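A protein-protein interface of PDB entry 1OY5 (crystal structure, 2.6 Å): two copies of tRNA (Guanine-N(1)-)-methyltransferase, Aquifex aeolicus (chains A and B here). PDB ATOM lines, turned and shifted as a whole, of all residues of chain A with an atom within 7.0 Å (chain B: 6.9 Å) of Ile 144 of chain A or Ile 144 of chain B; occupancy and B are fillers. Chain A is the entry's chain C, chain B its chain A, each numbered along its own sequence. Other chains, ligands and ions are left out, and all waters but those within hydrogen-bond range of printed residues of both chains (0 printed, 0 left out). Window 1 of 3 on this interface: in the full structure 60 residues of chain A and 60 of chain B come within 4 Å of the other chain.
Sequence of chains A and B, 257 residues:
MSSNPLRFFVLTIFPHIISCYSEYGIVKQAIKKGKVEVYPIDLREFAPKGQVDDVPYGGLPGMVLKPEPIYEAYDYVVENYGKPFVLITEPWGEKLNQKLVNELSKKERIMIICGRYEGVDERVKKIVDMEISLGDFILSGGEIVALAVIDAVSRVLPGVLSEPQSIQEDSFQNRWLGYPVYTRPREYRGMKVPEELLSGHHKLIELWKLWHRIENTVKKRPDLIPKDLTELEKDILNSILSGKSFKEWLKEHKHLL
The side-chain carboxylate (OD1) of Asp 151 of chain B lies within hydrogen-bond range of the backbone NH (N) of Ser 140 of chain A, at 2.8 Å.
The side-chain carboxylate (OD2) of Asp 151 of chain A sits at hydrogen-bond distance from the side-chain hydroxyl (OG) of Ser 140 of chain B (2.7 Å).
The side-chain hydroxyl (OH) of Tyr 21 of chain A is in hydrogen-bond range of the side-chain carboxylate (OD2) of Asp 151 of chain A (2.7 Å).
OH of Tyr 21 of chain B is in hydrogen-bond range of OD2 of Asp 151 of chain B (2.6 Å).
Ile 17 of chain A touches Tyr 21 of chain B (CD1 to CD2, 3.96 Å).
Tyr 21 of chain A touches Ile 17 of chain B.
Tyr 21 of chain A touches Ile 144 of chain B.
Ile 144 of chain A touches Tyr 21 of chain B (CD1 to OH, 3.0 Å).
CD1 of Ile 144 of chain A touches C of Leu 147 of chain B (3.7 Å).
Ala 148 of chain B touches Ile 144 of chain A.
Leu 147 of chain A touches Ile 144 of chain B (C to CD1, 3.7 Å).
Leu 139 of chain B touches Ala 148 of chain A (CD2 to O, 3.5 Å).
Ala 148 of chain A touches Ile 144 of chain B.
Leu 139 of chain B touches Asp 151 of chain A.
Of the printed residues of chain B, Leu 139 of chain A touches Ala 148 and Asp 151.
Of chain B, only Tyr 21 (3.0 Å), Ile 144 (3.6 Å), Leu 147 (3.7 Å), Ala 148 (3.7 Å) and Asp 151 (3.9 Å) come within 4 Å of Ile 144 of chain A.
Val 149 of chain A touches none of the printed residues of chain B.
Printed residues of chain A within 4 Å of Ile 17 of chain B: Tyr 21.
Printed residues of chain A within 4 Å of Tyr 21 of chain B: Ile 17 and Ile 144.
Of chain A, only Tyr 21 (2.9 Å), Ile 144 (3.6 Å), Leu 147 (3.7 Å), Ala 148 (3.6 Å) and Asp 151 (3.8 Å) come within 4 Å of Ile 144 of chain B.
Printed residues of chain A within 4 Å of Leu 147 of chain B: Ile 144 (3.7 Å).
Of the 20 printed residues of chain B, 8 touch a printed residue of chain A.
Printed residues of chain B that touch a printed residue of chain A: Ile 17, Tyr 21, Leu 139, Ser 140, Ile 144, Leu 147, Ala 148 and Asp 151.
Hydrophobic or aromatic side chains of chain B within 4 Å of the printed part of chain A: Ile 17, Tyr 21, Leu 139, Ile 144 and Ala 148.
Of the 21 printed residues of chain A, 8 touch a printed residue of chain B.
Printed residues of chain A that touch a printed residue of chain B: Ile 17, Tyr 21, Leu 139, Ser 140, Ile 144, Leu 147, Ala 148 and Asp 151.
Among the printed residues, 17 pairs touch across the chains.
Tyr 21 of chain A touches Ile 144 of chain B, and with the chains exchanged Ile 144 of chain A touches Tyr 21 of chain B.
Leu 139 of chain A touches Asp 151 of chain B, and with the chains exchanged Asp 151 of chain A touches Leu 139 of chain B.
Ile 144 of chain B touches its own counterpart, Ile 144 of chain A.
Ile 144 of chain A touches Ala 148 of chain B, and with the chains exchanged Ala 148 of chain A touches Ile 144 of chain B.
20 positions are printed for both chains.
Of the 17 pairs that touch across the chains among the printed residues, 17 have their exchanged pair printed and touching as well.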
ATOM      1  N   ILE A  17       2.377 -10.271 -16.833  1.00  0.00           N
ATOM      2  CA  ILE A  17       3.801 -10.492 -16.744  1.00  0.00           C
ATOM      3  C   ILE A  17       4.343  -9.851 -15.488  1.00  0.00           C
ATOM      4  O   ILE A  17       5.313 -10.329 -14.882  1.00  0.00           O
ATOM      5  CB  ILE A  17       4.511  -9.901 -17.987  1.00  0.00           C
ATOM      6  CG1 ILE A  17       4.480 -10.887 -19.139  1.00  0.00           C
ATOM      7  CG2 ILE A  17       5.936  -9.562 -17.716  1.00  0.00           C
ATOM      8  CD1 ILE A  17       4.864 -10.252 -20.499  1.00  0.00           C
ATOM      9  N   ILE A  18       3.705  -8.754 -15.098  1.00  0.00           N
ATOM     10  CA  ILE A  18       4.098  -8.020 -13.917  1.00  0.00           C
ATOM     11  C   ILE A  18       3.584  -8.761 -12.677  1.00  0.00           C
ATOM     12  O   ILE A  18       4.324  -8.998 -11.734  1.00  0.00           O
ATOM     13  CB  ILE A  18       3.600  -6.593 -14.023  1.00  0.00           C
ATOM     14  CG1 ILE A  18       3.989  -5.985 -15.394  1.00  0.00           C
ATOM     15  CG2 ILE A  18       4.182  -5.757 -12.946  1.00  0.00           C
ATOM     16  CD1 ILE A  18       5.518  -5.625 -15.574  1.00  0.00           C
ATOM     17  N   TYR A  21       5.815 -11.814 -12.056  1.00  0.00           N
ATOM     18  CA  TYR A  21       7.122 -11.581 -11.474  1.00  0.00           C
ATOM     19  C   TYR A  21       7.042 -11.191  -9.974  1.00  0.00           C
ATOM     20  O   TYR A  21       8.014 -11.384  -9.228  1.00  0.00           O
ATOM     21  CB  TYR A  21       7.860 -10.502 -12.236  1.00  0.00           C
ATOM     22  CG  TYR A  21       9.305 -10.446 -11.841  1.00  0.00           C
ATOM     23  CD1 TYR A  21       9.743  -9.562 -10.849  1.00  0.00           C
ATOM     24  CD2 TYR A  21      10.232 -11.346 -12.402  1.00  0.00           C
ATOM     25  CE1 TYR A  21      11.061  -9.543 -10.450  1.00  0.00           C
ATOM     26  CE2 TYR A  21      11.560 -11.325 -12.034  1.00  0.00           C
ATOM     27  CZ  TYR A  21      11.973 -10.426 -11.053  1.00  0.00           C
ATOM     28  OH  TYR A  21      13.287 -10.428 -10.666  1.00  0.00           O
ATOM     29  N   VAL A  27      10.731  -9.495  -4.711  1.00  0.00           N
ATOM     30  CA  VAL A  27       9.585  -8.630  -4.883  1.00  0.00           C
ATOM     31  C   VAL A  27       8.426  -9.180  -4.014  1.00  0.00           C
ATOM     32  O   VAL A  27       7.695  -8.433  -3.328  1.00  0.00           O
ATOM     33  CB  VAL A  27       9.171  -8.509  -6.377  1.00  0.00           C
ATOM     34  CG1 VAL A  27       7.943  -7.576  -6.525  1.00  0.00           C
ATOM     35  CG2 VAL A  27      10.324  -7.936  -7.211  1.00  0.00           C
ATOM     36  N   THR A  89      10.150   3.377 -19.791  1.00  0.00           N
ATOM     37  CA  THR A  89      11.093   2.419 -20.323  1.00  0.00           C
ATOM     38  C   THR A  89      10.749   2.136 -21.779  1.00  0.00           C
ATOM     39  O   THR A  89       9.748   1.487 -22.079  1.00  0.00           O
ATOM     40  CB  THR A  89      11.103   1.095 -19.513  1.00  0.00           C
ATOM     41  OG1 THR A  89       9.806   0.470 -19.527  1.00  0.00           O
ATOM     42  CG2 THR A  89      11.343   1.355 -18.048  1.00  0.00           C
ATOM     43  N   CYS A 114       5.662   1.280 -19.887  1.00  0.00           N
ATOM     44  CA  CYS A 114       6.423   0.296 -20.637  1.00  0.00           C
ATOM     45  C   CYS A 114       6.263   0.621 -22.073  1.00  0.00           C
ATOM     46  O   CYS A 114       5.173   0.470 -22.598  1.00  0.00           O
ATOM     47  CB  CYS A 114       5.898  -1.111 -20.365  1.00  0.00           C
ATOM     48  SG  CYS A 114       5.960  -1.570 -18.601  1.00  0.00           S
ATOM     49  N   PHE A 137      21.231  -2.676 -26.645  1.00  0.00           N
ATOM     50  CA  PHE A 137      20.624  -3.836 -27.305  1.00  0.00           C
ATOM     51  C   PHE A 137      19.130  -3.555 -27.393  1.00  0.00           C
ATOM     52  O   PHE A 137      18.645  -2.691 -26.725  1.00  0.00           O
ATOM     53  CB  PHE A 137      20.949  -5.161 -26.561  1.00  0.00           C
ATOM     54  CG  PHE A 137      20.260  -5.304 -25.210  1.00  0.00           C
ATOM     55  CD1 PHE A 137      20.744  -4.666 -24.102  1.00  0.00           C
ATOM     56  CD2 PHE A 137      19.142  -6.095 -25.075  1.00  0.00           C
ATOM     57  CE1 PHE A 137      20.118  -4.798 -22.889  1.00  0.00           C
ATOM     58  CE2 PHE A 137      18.515  -6.229 -23.888  1.00  0.00           C
ATOM     59  CZ  PHE A 137      18.992  -5.576 -22.773  1.00  0.00           C
ATOM     60  N   LEU A 139      15.112  -4.645 -27.103  1.00  0.00           N
ATOM     61  CA  LEU A 139      14.052  -5.487 -26.621  1.00  0.00           C
ATOM     62  C   LEU A 139      12.794  -5.104 -27.407  1.00  0.00           C
ATOM     63  O   LEU A 139      12.802  -4.130 -28.142  1.00  0.00           O
ATOM     64  CB  LEU A 139      13.854  -5.241 -25.129  1.00  0.00           C
ATOM     65  CG  LEU A 139      15.009  -5.708 -24.270  1.00  0.00           C
ATOM     66  CD1 LEU A 139      14.876  -5.225 -22.888  1.00  0.00           C
ATOM     67  CD2 LEU A 139      15.021  -7.195 -24.266  1.00  0.00           C
ATOM     68  N   SER A 140      11.733  -5.873 -27.265  1.00  0.00           N
ATOM     69  CA  SER A 140      10.472  -5.570 -27.909  1.00  0.00           C
ATOM     70  C   SER A 140       9.532  -4.733 -27.054  1.00  0.00           C
ATOM     71  O   SER A 140       8.433  -4.427 -27.465  1.00  0.00           O
ATOM     72  CB  SER A 140       9.756  -6.883 -28.224  1.00  0.00           C
ATOM     73  OG  SER A 140       9.313  -7.547 -27.020  1.00  0.00           O
ATOM     74  N   GLY A 141       9.937  -4.369 -25.852  1.00  0.00           N
ATOM     75  CA  GLY A 141       9.043  -3.641 -24.980  1.00  0.00           C
ATOM     76  C   GLY A 141       9.714  -3.347 -23.668  1.00  0.00           C
ATOM     77  O   GLY A 141      10.790  -3.875 -23.409  1.00  0.00           O
ATOM     78  N   GLY A 142       9.064  -2.550 -22.839  1.00  0.00           N
ATOM     79  CA  GLY A 142       9.667  -2.067 -21.613  1.00  0.00           C
ATOM     80  C   GLY A 142       9.430  -2.883 -20.371  1.00  0.00           C
ATOM     81  O   GLY A 142      10.025  -2.610 -19.314  1.00  0.00           O
ATOM     82  N   GLU A 143       8.591  -3.896 -20.480  1.00  0.00           N
ATOM     83  CA  GLU A 143       8.292  -4.736 -19.330  1.00  0.00           C
ATOM     84  C   GLU A 143       9.523  -5.202 -18.552  1.00  0.00           C
ATOM     85  O   GLU A 143       9.586  -5.002 -17.352  1.00  0.00           O
ATOM     86  CB  GLU A 143       7.457  -5.934 -19.758  1.00  0.00           C
ATOM     87  CG  GLU A 143       6.039  -5.554 -20.089  1.00  0.00           C
ATOM     88  CD  GLU A 143       5.899  -4.760 -21.373  1.00  0.00           C
ATOM     89  OE1 GLU A 143       4.909  -4.029 -21.525  1.00  0.00           O
ATOM     90  OE2 GLU A 143       6.765  -4.863 -22.236  1.00  0.00           O
ATOM     91  N   ILE A 144      10.478  -5.825 -19.245  1.00  0.00           N
ATOM     92  CA  ILE A 144      11.680  -6.447 -18.630  1.00  0.00           C
ATOM     93  C   ILE A 144      12.472  -5.432 -17.808  1.00  0.00           C
ATOM     94  O   ILE A 144      12.893  -5.720 -16.672  1.00  0.00           O
ATOM     95  CB  ILE A 144      12.541  -7.160 -19.716  1.00  0.00           C
ATOM     96  CG1 ILE A 144      11.843  -8.452 -20.133  1.00  0.00           C
ATOM     97  CG2 ILE A 144      13.924  -7.499 -19.231  1.00  0.00           C
ATOM     98  CD1 ILE A 144      12.407  -9.104 -21.378  1.00  0.00           C
ATOM     99  N   VAL A 145      12.603  -4.222 -18.361  1.00  0.00           N
ATOM    100  CA  VAL A 145      13.247  -3.092 -17.660  1.00  0.00           C
ATOM    101  C   VAL A 145      12.453  -2.665 -16.470  1.00  0.00           C
ATOM    102  O   VAL A 145      13.012  -2.370 -15.440  1.00  0.00           O
ATOM    103  CB  VAL A 145      13.416  -1.900 -18.563  1.00  0.00           C
ATOM    104  CG1 VAL A 145      14.050  -0.738 -17.826  1.00  0.00           C
ATOM    105  CG2 VAL A 145      14.287  -2.299 -19.716  1.00  0.00           C
ATOM    106  N   ALA A 146      11.135  -2.655 -16.595  1.00  0.00           N
ATOM    107  CA  ALA A 146      10.271  -2.307 -15.462  1.00  0.00           C
ATOM    108  C   ALA A 146      10.506  -3.258 -14.308  1.00  0.00           C
ATOM    109  O   ALA A 146      10.643  -2.841 -13.186  1.00  0.00           O
ATOM    110  CB  ALA A 146       8.877  -2.364 -15.858  1.00  0.00           C
ATOM    111  N   LEU A 147      10.546  -4.550 -14.599  1.00  0.00           N
ATOM    112  CA  LEU A 147      10.795  -5.583 -13.603  1.00  0.00           C
ATOM    113  C   LEU A 147      12.163  -5.420 -12.980  1.00  0.00           C
ATOM    114  O   LEU A 147      12.277  -5.455 -11.755  1.00  0.00           O
ATOM    115  CB  LEU A 147      10.679  -6.981 -14.234  1.00  0.00           C
ATOM    116  CG  LEU A 147       9.301  -7.271 -14.784  1.00  0.00           C
ATOM    117  CD1 LEU A 147       9.187  -8.609 -15.468  1.00  0.00           C
ATOM    118  CD2 LEU A 147       8.271  -7.161 -13.616  1.00  0.00           C
ATOM    119  N   ALA A 148      13.191  -5.258 -13.806  1.00  0.00           N
ATOM    120  CA  ALA A 148      14.542  -4.960 -13.314  1.00  0.00           C
ATOM    121  C   ALA A 148      14.513  -3.799 -12.325  1.00  0.00           C
ATOM    122  O   ALA A 148      15.194  -3.843 -11.308  1.00  0.00           O
ATOM    123  CB  ALA A 148      15.489  -4.624 -14.471  1.00  0.00           C
ATOM    124  N   VAL A 149      13.724  -2.765 -12.628  1.00  0.00           N
ATOM    125  CA  VAL A 149      13.643  -1.590 -11.753  1.00  0.00           C
ATOM    126  C   VAL A 149      13.025  -2.005 -10.425  1.00  0.00           C
ATOM    127  O   VAL A 149      13.640  -1.878  -9.364  1.00  0.00           O
ATOM    128  CB  VAL A 149      12.822  -0.444 -12.409  1.00  0.00           C
ATOM    129  CG1 VAL A 149      12.508   0.664 -11.422  1.00  0.00           C
ATOM    130  CG2 VAL A 149      13.579   0.140 -13.592  1.00  0.00           C
ATOM    131  N   ILE A 150      11.810  -2.530 -10.536  1.00  0.00           N
ATOM    132  CA  ILE A 150      11.057  -3.073  -9.416  1.00  0.00           C
ATOM    133  C   ILE A 150      11.929  -4.023  -8.594  1.00  0.00           C
ATOM    134  O   ILE A 150      11.900  -4.008  -7.379  1.00  0.00           O
ATOM    135  CB  ILE A 150       9.791  -3.806  -9.928  1.00  0.00           C
ATOM    136  CG1 ILE A 150       8.868  -2.806 -10.649  1.00  0.00           C
ATOM    137  CG2 ILE A 150       9.052  -4.486  -8.778  1.00  0.00           C
ATOM    138  CD1 ILE A 150       7.651  -3.424 -11.253  1.00  0.00           C
ATOM    139  N   ASP A 151      12.731  -4.825  -9.266  1.00  0.00           N
ATOM    140  CA  ASP A 151      13.558  -5.761  -8.556  1.00  0.00           C
ATOM    141  C   ASP A 151      14.639  -5.002  -7.793  1.00  0.00           C
ATOM    142  O   ASP A 151      14.775  -5.136  -6.572  1.00  0.00           O
ATOM    143  CB  ASP A 151      14.138  -6.768  -9.537  1.00  0.00           C
ATOM    144  CG  ASP A 151      14.909  -7.870  -8.873  1.00  0.00           C
ATOM    145  OD1 ASP A 151      16.078  -7.662  -8.518  1.00  0.00           O
ATOM    146  OD2 ASP A 151      14.470  -9.023  -8.709  1.00  0.00           O
ATOM    147  N   ALA A 152      15.415  -4.204  -8.514  1.00  0.00           N
ATOM    148  CA  ALA A 152      16.529  -3.492  -7.895  1.00  0.00           C
ATOM    149  C   ALA A 152      16.065  -2.613  -6.712  1.00  0.00           C
ATOM    150  O   ALA A 152      16.611  -2.632  -5.618  1.00  0.00           O
ATOM    151  CB  ALA A 152      17.258  -2.667  -8.919  1.00  0.00           C
ATOM    152  N   ILE B  17       8.255 -17.830 -13.825  1.00  0.00           N
ATOM    153  CA  ILE B  17       8.572 -16.513 -14.334  1.00  0.00           C
ATOM    154  C   ILE B  17       8.854 -16.621 -15.827  1.00  0.00           C
ATOM    155  O   ILE B  17       8.373 -15.814 -16.600  1.00  0.00           O
ATOM    156  CB  ILE B  17       9.742 -15.883 -13.591  1.00  0.00           C
ATOM    157  CG1 ILE B  17       9.287 -15.377 -12.234  1.00  0.00           C
ATOM    158  CG2 ILE B  17      10.265 -14.718 -14.360  1.00  0.00           C
ATOM    159  CD1 ILE B  17      10.403 -15.206 -11.227  1.00  0.00           C
ATOM    160  N   ILE B  18       9.600 -17.636 -16.226  1.00  0.00           N
ATOM    161  CA  ILE B  18       9.959 -17.822 -17.614  1.00  0.00           C
ATOM    162  C   ILE B  18       8.738 -18.267 -18.445  1.00  0.00           C
ATOM    163  O   ILE B  18       8.468 -17.743 -19.518  1.00  0.00           O
ATOM    164  CB  ILE B  18      11.077 -18.837 -17.706  1.00  0.00           C
ATOM    165  CG1 ILE B  18      12.155 -18.527 -16.671  1.00  0.00           C
ATOM    166  CG2 ILE B  18      11.644 -18.904 -19.128  1.00  0.00           C
ATOM    167  CD1 ILE B  18      12.814 -17.246 -16.851  1.00  0.00           C
ATOM    168  N   TYR B  21       6.483 -15.299 -19.160  1.00  0.00           N
ATOM    169  CA  TYR B  21       6.922 -14.249 -20.094  1.00  0.00           C
ATOM    170  C   TYR B  21       6.759 -14.748 -21.501  1.00  0.00           C
ATOM    171  O   TYR B  21       6.603 -13.958 -22.395  1.00  0.00           O
ATOM    172  CB  TYR B  21       8.375 -13.829 -19.846  1.00  0.00           C
ATOM    173  CG  TYR B  21       8.814 -12.616 -20.672  1.00  0.00           C
ATOM    174  CD1 TYR B  21       9.352 -12.779 -21.930  1.00  0.00           C
ATOM    175  CD2 TYR B  21       8.668 -11.314 -20.191  1.00  0.00           C
ATOM    176  CE1 TYR B  21       9.723 -11.739 -22.677  1.00  0.00           C
ATOM    177  CE2 TYR B  21       9.033 -10.253 -20.928  1.00  0.00           C
ATOM    178  CZ  TYR B  21       9.568 -10.462 -22.191  1.00  0.00           C
ATOM    179  OH  TYR B  21       9.949  -9.404 -23.008  1.00  0.00           O
ATOM    180  N   THR B  89      23.931 -15.805 -16.198  1.00  0.00           N
ATOM    181  CA  THR B  89      23.633 -14.449 -15.788  1.00  0.00           C
ATOM    182  C   THR B  89      23.658 -14.483 -14.280  1.00  0.00           C
ATOM    183  O   THR B  89      22.829 -15.176 -13.651  1.00  0.00           O
ATOM    184  CB  THR B  89      22.219 -14.062 -16.166  1.00  0.00           C
ATOM    185  OG1 THR B  89      21.305 -14.971 -15.530  1.00  0.00           O
ATOM    186  CG2 THR B  89      21.940 -14.237 -17.651  1.00  0.00           C
ATOM    187  N   CYS B 114      20.432 -19.262 -14.337  1.00  0.00           N
ATOM    188  CA  CYS B 114      20.028 -18.051 -13.662  1.00  0.00           C
ATOM    189  C   CYS B 114      20.636 -17.992 -12.271  1.00  0.00           C
ATOM    190  O   CYS B 114      20.346 -18.797 -11.451  1.00  0.00           O
ATOM    191  CB  CYS B 114      18.503 -17.927 -13.605  1.00  0.00           C
ATOM    192  SG  CYS B 114      17.682 -17.787 -15.202  1.00  0.00           S
ATOM    193  N   PHE B 137      24.248  -2.127 -11.672  1.00  0.00           N
ATOM    194  CA  PHE B 137      23.141  -2.201 -10.726  1.00  0.00           C
ATOM    195  C   PHE B 137      23.002  -3.691 -10.336  1.00  0.00           C
ATOM    196  O   PHE B 137      23.589  -4.555 -10.974  1.00  0.00           O
ATOM    197  CB  PHE B 137      21.845  -1.613 -11.302  1.00  0.00           C
ATOM    198  CG  PHE B 137      21.162  -2.494 -12.304  1.00  0.00           C
ATOM    199  CD1 PHE B 137      21.592  -2.530 -13.609  1.00  0.00           C
ATOM    200  CD2 PHE B 137      20.090  -3.286 -11.930  1.00  0.00           C
ATOM    201  CE1 PHE B 137      20.969  -3.333 -14.525  1.00  0.00           C
ATOM    202  CE2 PHE B 137      19.457  -4.090 -12.829  1.00  0.00           C
ATOM    203  CZ  PHE B 137      19.884  -4.138 -14.129  1.00  0.00           C
ATOM    204  N   LEU B 139      20.679  -7.069  -9.150  1.00  0.00           N
ATOM    205  CA  LEU B 139      19.391  -7.728  -9.168  1.00  0.00           C
ATOM    206  C   LEU B 139      19.439  -8.854  -8.159  1.00  0.00           C
ATOM    207  O   LEU B 139      20.501  -9.222  -7.675  1.00  0.00           O
ATOM    208  CB  LEU B 139      19.103  -8.253 -10.549  1.00  0.00           C
ATOM    209  CG  LEU B 139      18.752  -7.176 -11.588  1.00  0.00           C
ATOM    210  CD1 LEU B 139      18.689  -7.739 -12.963  1.00  0.00           C
ATOM    211  CD2 LEU B 139      17.417  -6.531 -11.254  1.00  0.00           C
ATOM    212  N   SER B 140      18.285  -9.382  -7.797  1.00  0.00           N
ATOM    213  CA  SER B 140      18.253 -10.450  -6.822  1.00  0.00           C
ATOM    214  C   SER B 140      18.370 -11.795  -7.525  1.00  0.00           C
ATOM    215  O   SER B 140      18.514 -12.797  -6.871  1.00  0.00           O
ATOM    216  CB  SER B 140      16.997 -10.365  -5.980  1.00  0.00           C
ATOM    217  OG  SER B 140      15.865 -10.234  -6.795  1.00  0.00           O
ATOM    218  N   GLY B 141      18.338 -11.808  -8.849  1.00  0.00           N
ATOM    219  CA  GLY B 141      18.507 -13.035  -9.610  1.00  0.00           C
ATOM    220  C   GLY B 141      18.618 -12.802 -11.108  1.00  0.00           C
ATOM    221  O   GLY B 141      18.282 -11.717 -11.602  1.00  0.00           O
ATOM    222  N   GLY B 142      19.034 -13.850 -11.824  1.00  0.00           N
ATOM    223  CA  GLY B 142      19.293 -13.822 -13.263  1.00  0.00           C
ATOM    224  C   GLY B 142      18.108 -14.030 -14.156  1.00  0.00           C
ATOM    225  O   GLY B 142      18.218 -14.012 -15.363  1.00  0.00           O
ATOM    226  N   GLU B 143      16.949 -14.233 -13.576  1.00  0.00           N
ATOM    227  CA  GLU B 143      15.756 -14.459 -14.375  1.00  0.00           C
ATOM    228  C   GLU B 143      15.502 -13.326 -15.380  1.00  0.00           C
ATOM    229  O   GLU B 143      15.254 -13.556 -16.532  1.00  0.00           O
ATOM    230  CB  GLU B 143      14.544 -14.636 -13.464  1.00  0.00           C
ATOM    231  CG  GLU B 143      14.434 -15.995 -12.877  1.00  0.00           C
ATOM    232  CD  GLU B 143      15.408 -16.300 -11.753  1.00  0.00           C
ATOM    233  OE1 GLU B 143      15.494 -17.478 -11.378  1.00  0.00           O
ATOM    234  OE2 GLU B 143      16.072 -15.420 -11.190  1.00  0.00           O
ATOM    235  N   ILE B 144      15.505 -12.103 -14.899  1.00  0.00           N
ATOM    236  CA  ILE B 144      15.258 -10.928 -15.719  1.00  0.00           C
ATOM    237  C   ILE B 144      16.266 -10.774 -16.870  1.00  0.00           C
ATOM    238  O   ILE B 144      15.941 -10.234 -17.925  1.00  0.00           O
ATOM    239  CB  ILE B 144      15.299  -9.672 -14.784  1.00  0.00           C
ATOM    240  CG1 ILE B 144      13.994  -9.560 -14.013  1.00  0.00           C
ATOM    241  CG2 ILE B 144      15.502  -8.434 -15.541  1.00  0.00           C
ATOM    242  CD1 ILE B 144      14.079  -8.592 -12.827  1.00  0.00           C
ATOM    243  N   VAL B 145      17.481 -11.251 -16.668  1.00  0.00           N
ATOM    244  CA  VAL B 145      18.517 -11.125 -17.666  1.00  0.00           C
ATOM    245  C   VAL B 145      18.341 -12.221 -18.667  1.00  0.00           C
ATOM    246  O   VAL B 145      18.592 -12.050 -19.875  1.00  0.00           O
ATOM    247  CB  VAL B 145      19.913 -11.138 -17.050  1.00  0.00           C
ATOM    248  CG1 VAL B 145      20.971 -11.295 -18.115  1.00  0.00           C
ATOM    249  CG2 VAL B 145      20.138  -9.818 -16.261  1.00  0.00           C
ATOM    250  N   ALA B 146      17.861 -13.342 -18.174  1.00  0.00           N
ATOM    251  CA  ALA B 146      17.586 -14.464 -19.061  1.00  0.00           C
ATOM    252  C   ALA B 146      16.478 -14.068 -20.016  1.00  0.00           C
ATOM    253  O   ALA B 146      16.554 -14.359 -21.223  1.00  0.00           O
ATOM    254  CB  ALA B 146      17.179 -15.703 -18.258  1.00  0.00           C
ATOM    255  N   LEU B 147      15.446 -13.413 -19.489  1.00  0.00           N
ATOM    256  CA  LEU B 147      14.305 -13.068 -20.313  1.00  0.00           C
ATOM    257  C   LEU B 147      14.737 -12.027 -21.370  1.00  0.00           C
ATOM    258  O   LEU B 147      14.432 -12.162 -22.567  1.00  0.00           O
ATOM    259  CB  LEU B 147      13.143 -12.602 -19.459  1.00  0.00           C
ATOM    260  CG  LEU B 147      12.442 -13.614 -18.525  1.00  0.00           C
ATOM    261  CD1 LEU B 147      11.391 -12.892 -17.692  1.00  0.00           C
ATOM    262  CD2 LEU B 147      11.782 -14.718 -19.282  1.00  0.00           C
ATOM    263  N   ALA B 148      15.501 -11.029 -20.933  1.00  0.00           N
ATOM    264  CA  ALA B 148      16.015 -10.048 -21.852  1.00  0.00           C
ATOM    265  C   ALA B 148      16.734 -10.764 -22.996  1.00  0.00           C
ATOM    266  O   ALA B 148      16.458 -10.533 -24.158  1.00  0.00           O
ATOM    267  CB  ALA B 148      16.952  -9.143 -21.144  1.00  0.00           C
ATOM    268  N   VAL B 149      17.628 -11.676 -22.656  1.00  0.00           N
ATOM    269  CA  VAL B 149      18.342 -12.428 -23.667  1.00  0.00           C
ATOM    270  C   VAL B 149      17.367 -13.182 -24.634  1.00  0.00           C
ATOM    271  O   VAL B 149      17.541 -13.148 -25.848  1.00  0.00           O
ATOM    272  CB  VAL B 149      19.318 -13.412 -23.017  1.00  0.00           C
ATOM    273  CG1 VAL B 149      19.877 -14.345 -24.041  1.00  0.00           C
ATOM    274  CG2 VAL B 149      20.451 -12.682 -22.333  1.00  0.00           C
ATOM    275  N   ILE B 150      16.360 -13.864 -24.069  1.00  0.00           N
ATOM    276  CA  ILE B 150      15.382 -14.592 -24.869  1.00  0.00           C
ATOM    277  C   ILE B 150      14.613 -13.638 -25.784  1.00  0.00           C
ATOM    278  O   ILE B 150      14.362 -13.936 -26.946  1.00  0.00           O
ATOM    279  CB  ILE B 150      14.421 -15.351 -23.951  1.00  0.00           C
ATOM    280  CG1 ILE B 150      15.159 -16.495 -23.238  1.00  0.00           C
ATOM    281  CG2 ILE B 150      13.323 -15.981 -24.756  1.00  0.00           C
ATOM    282  CD1 ILE B 150      14.335 -17.273 -22.248  1.00  0.00           C
ATOM    283  N   ASP B 151      14.253 -12.476 -25.229  1.00  0.00           N
ATOM    284  CA  ASP B 151      13.517 -11.443 -25.946  1.00  0.00           C
ATOM    285  C   ASP B 151      14.338 -10.872 -27.089  1.00  0.00           C
ATOM    286  O   ASP B 151      13.880 -10.811 -28.207  1.00  0.00           O
ATOM    287  CB  ASP B 151      13.123 -10.325 -24.978  1.00  0.00           C
ATOM    288  CG  ASP B 151      12.140  -9.346 -25.575  1.00  0.00           C
ATOM    289  OD1 ASP B 151      12.570  -8.390 -26.242  1.00  0.00           O
ATOM    290  OD2 ASP B 151      10.910  -9.399 -25.382  1.00  0.00           O
ATOM    291  N   ALA B 152      15.557 -10.445 -26.792  1.00  0.00           N
ATOM    292  CA  ALA B 152      16.417  -9.799 -27.777  1.00  0.00           C
ATOM    293  C   ALA B 152      16.716 -10.699 -28.967  1.00  0.00           C
ATOM    294  O   ALA B 152      16.640 -10.274 -30.123  1.00  0.00           O
ATOM    295  CB  ALA B 152      17.732  -9.327 -27.122  1.00  0.00           C
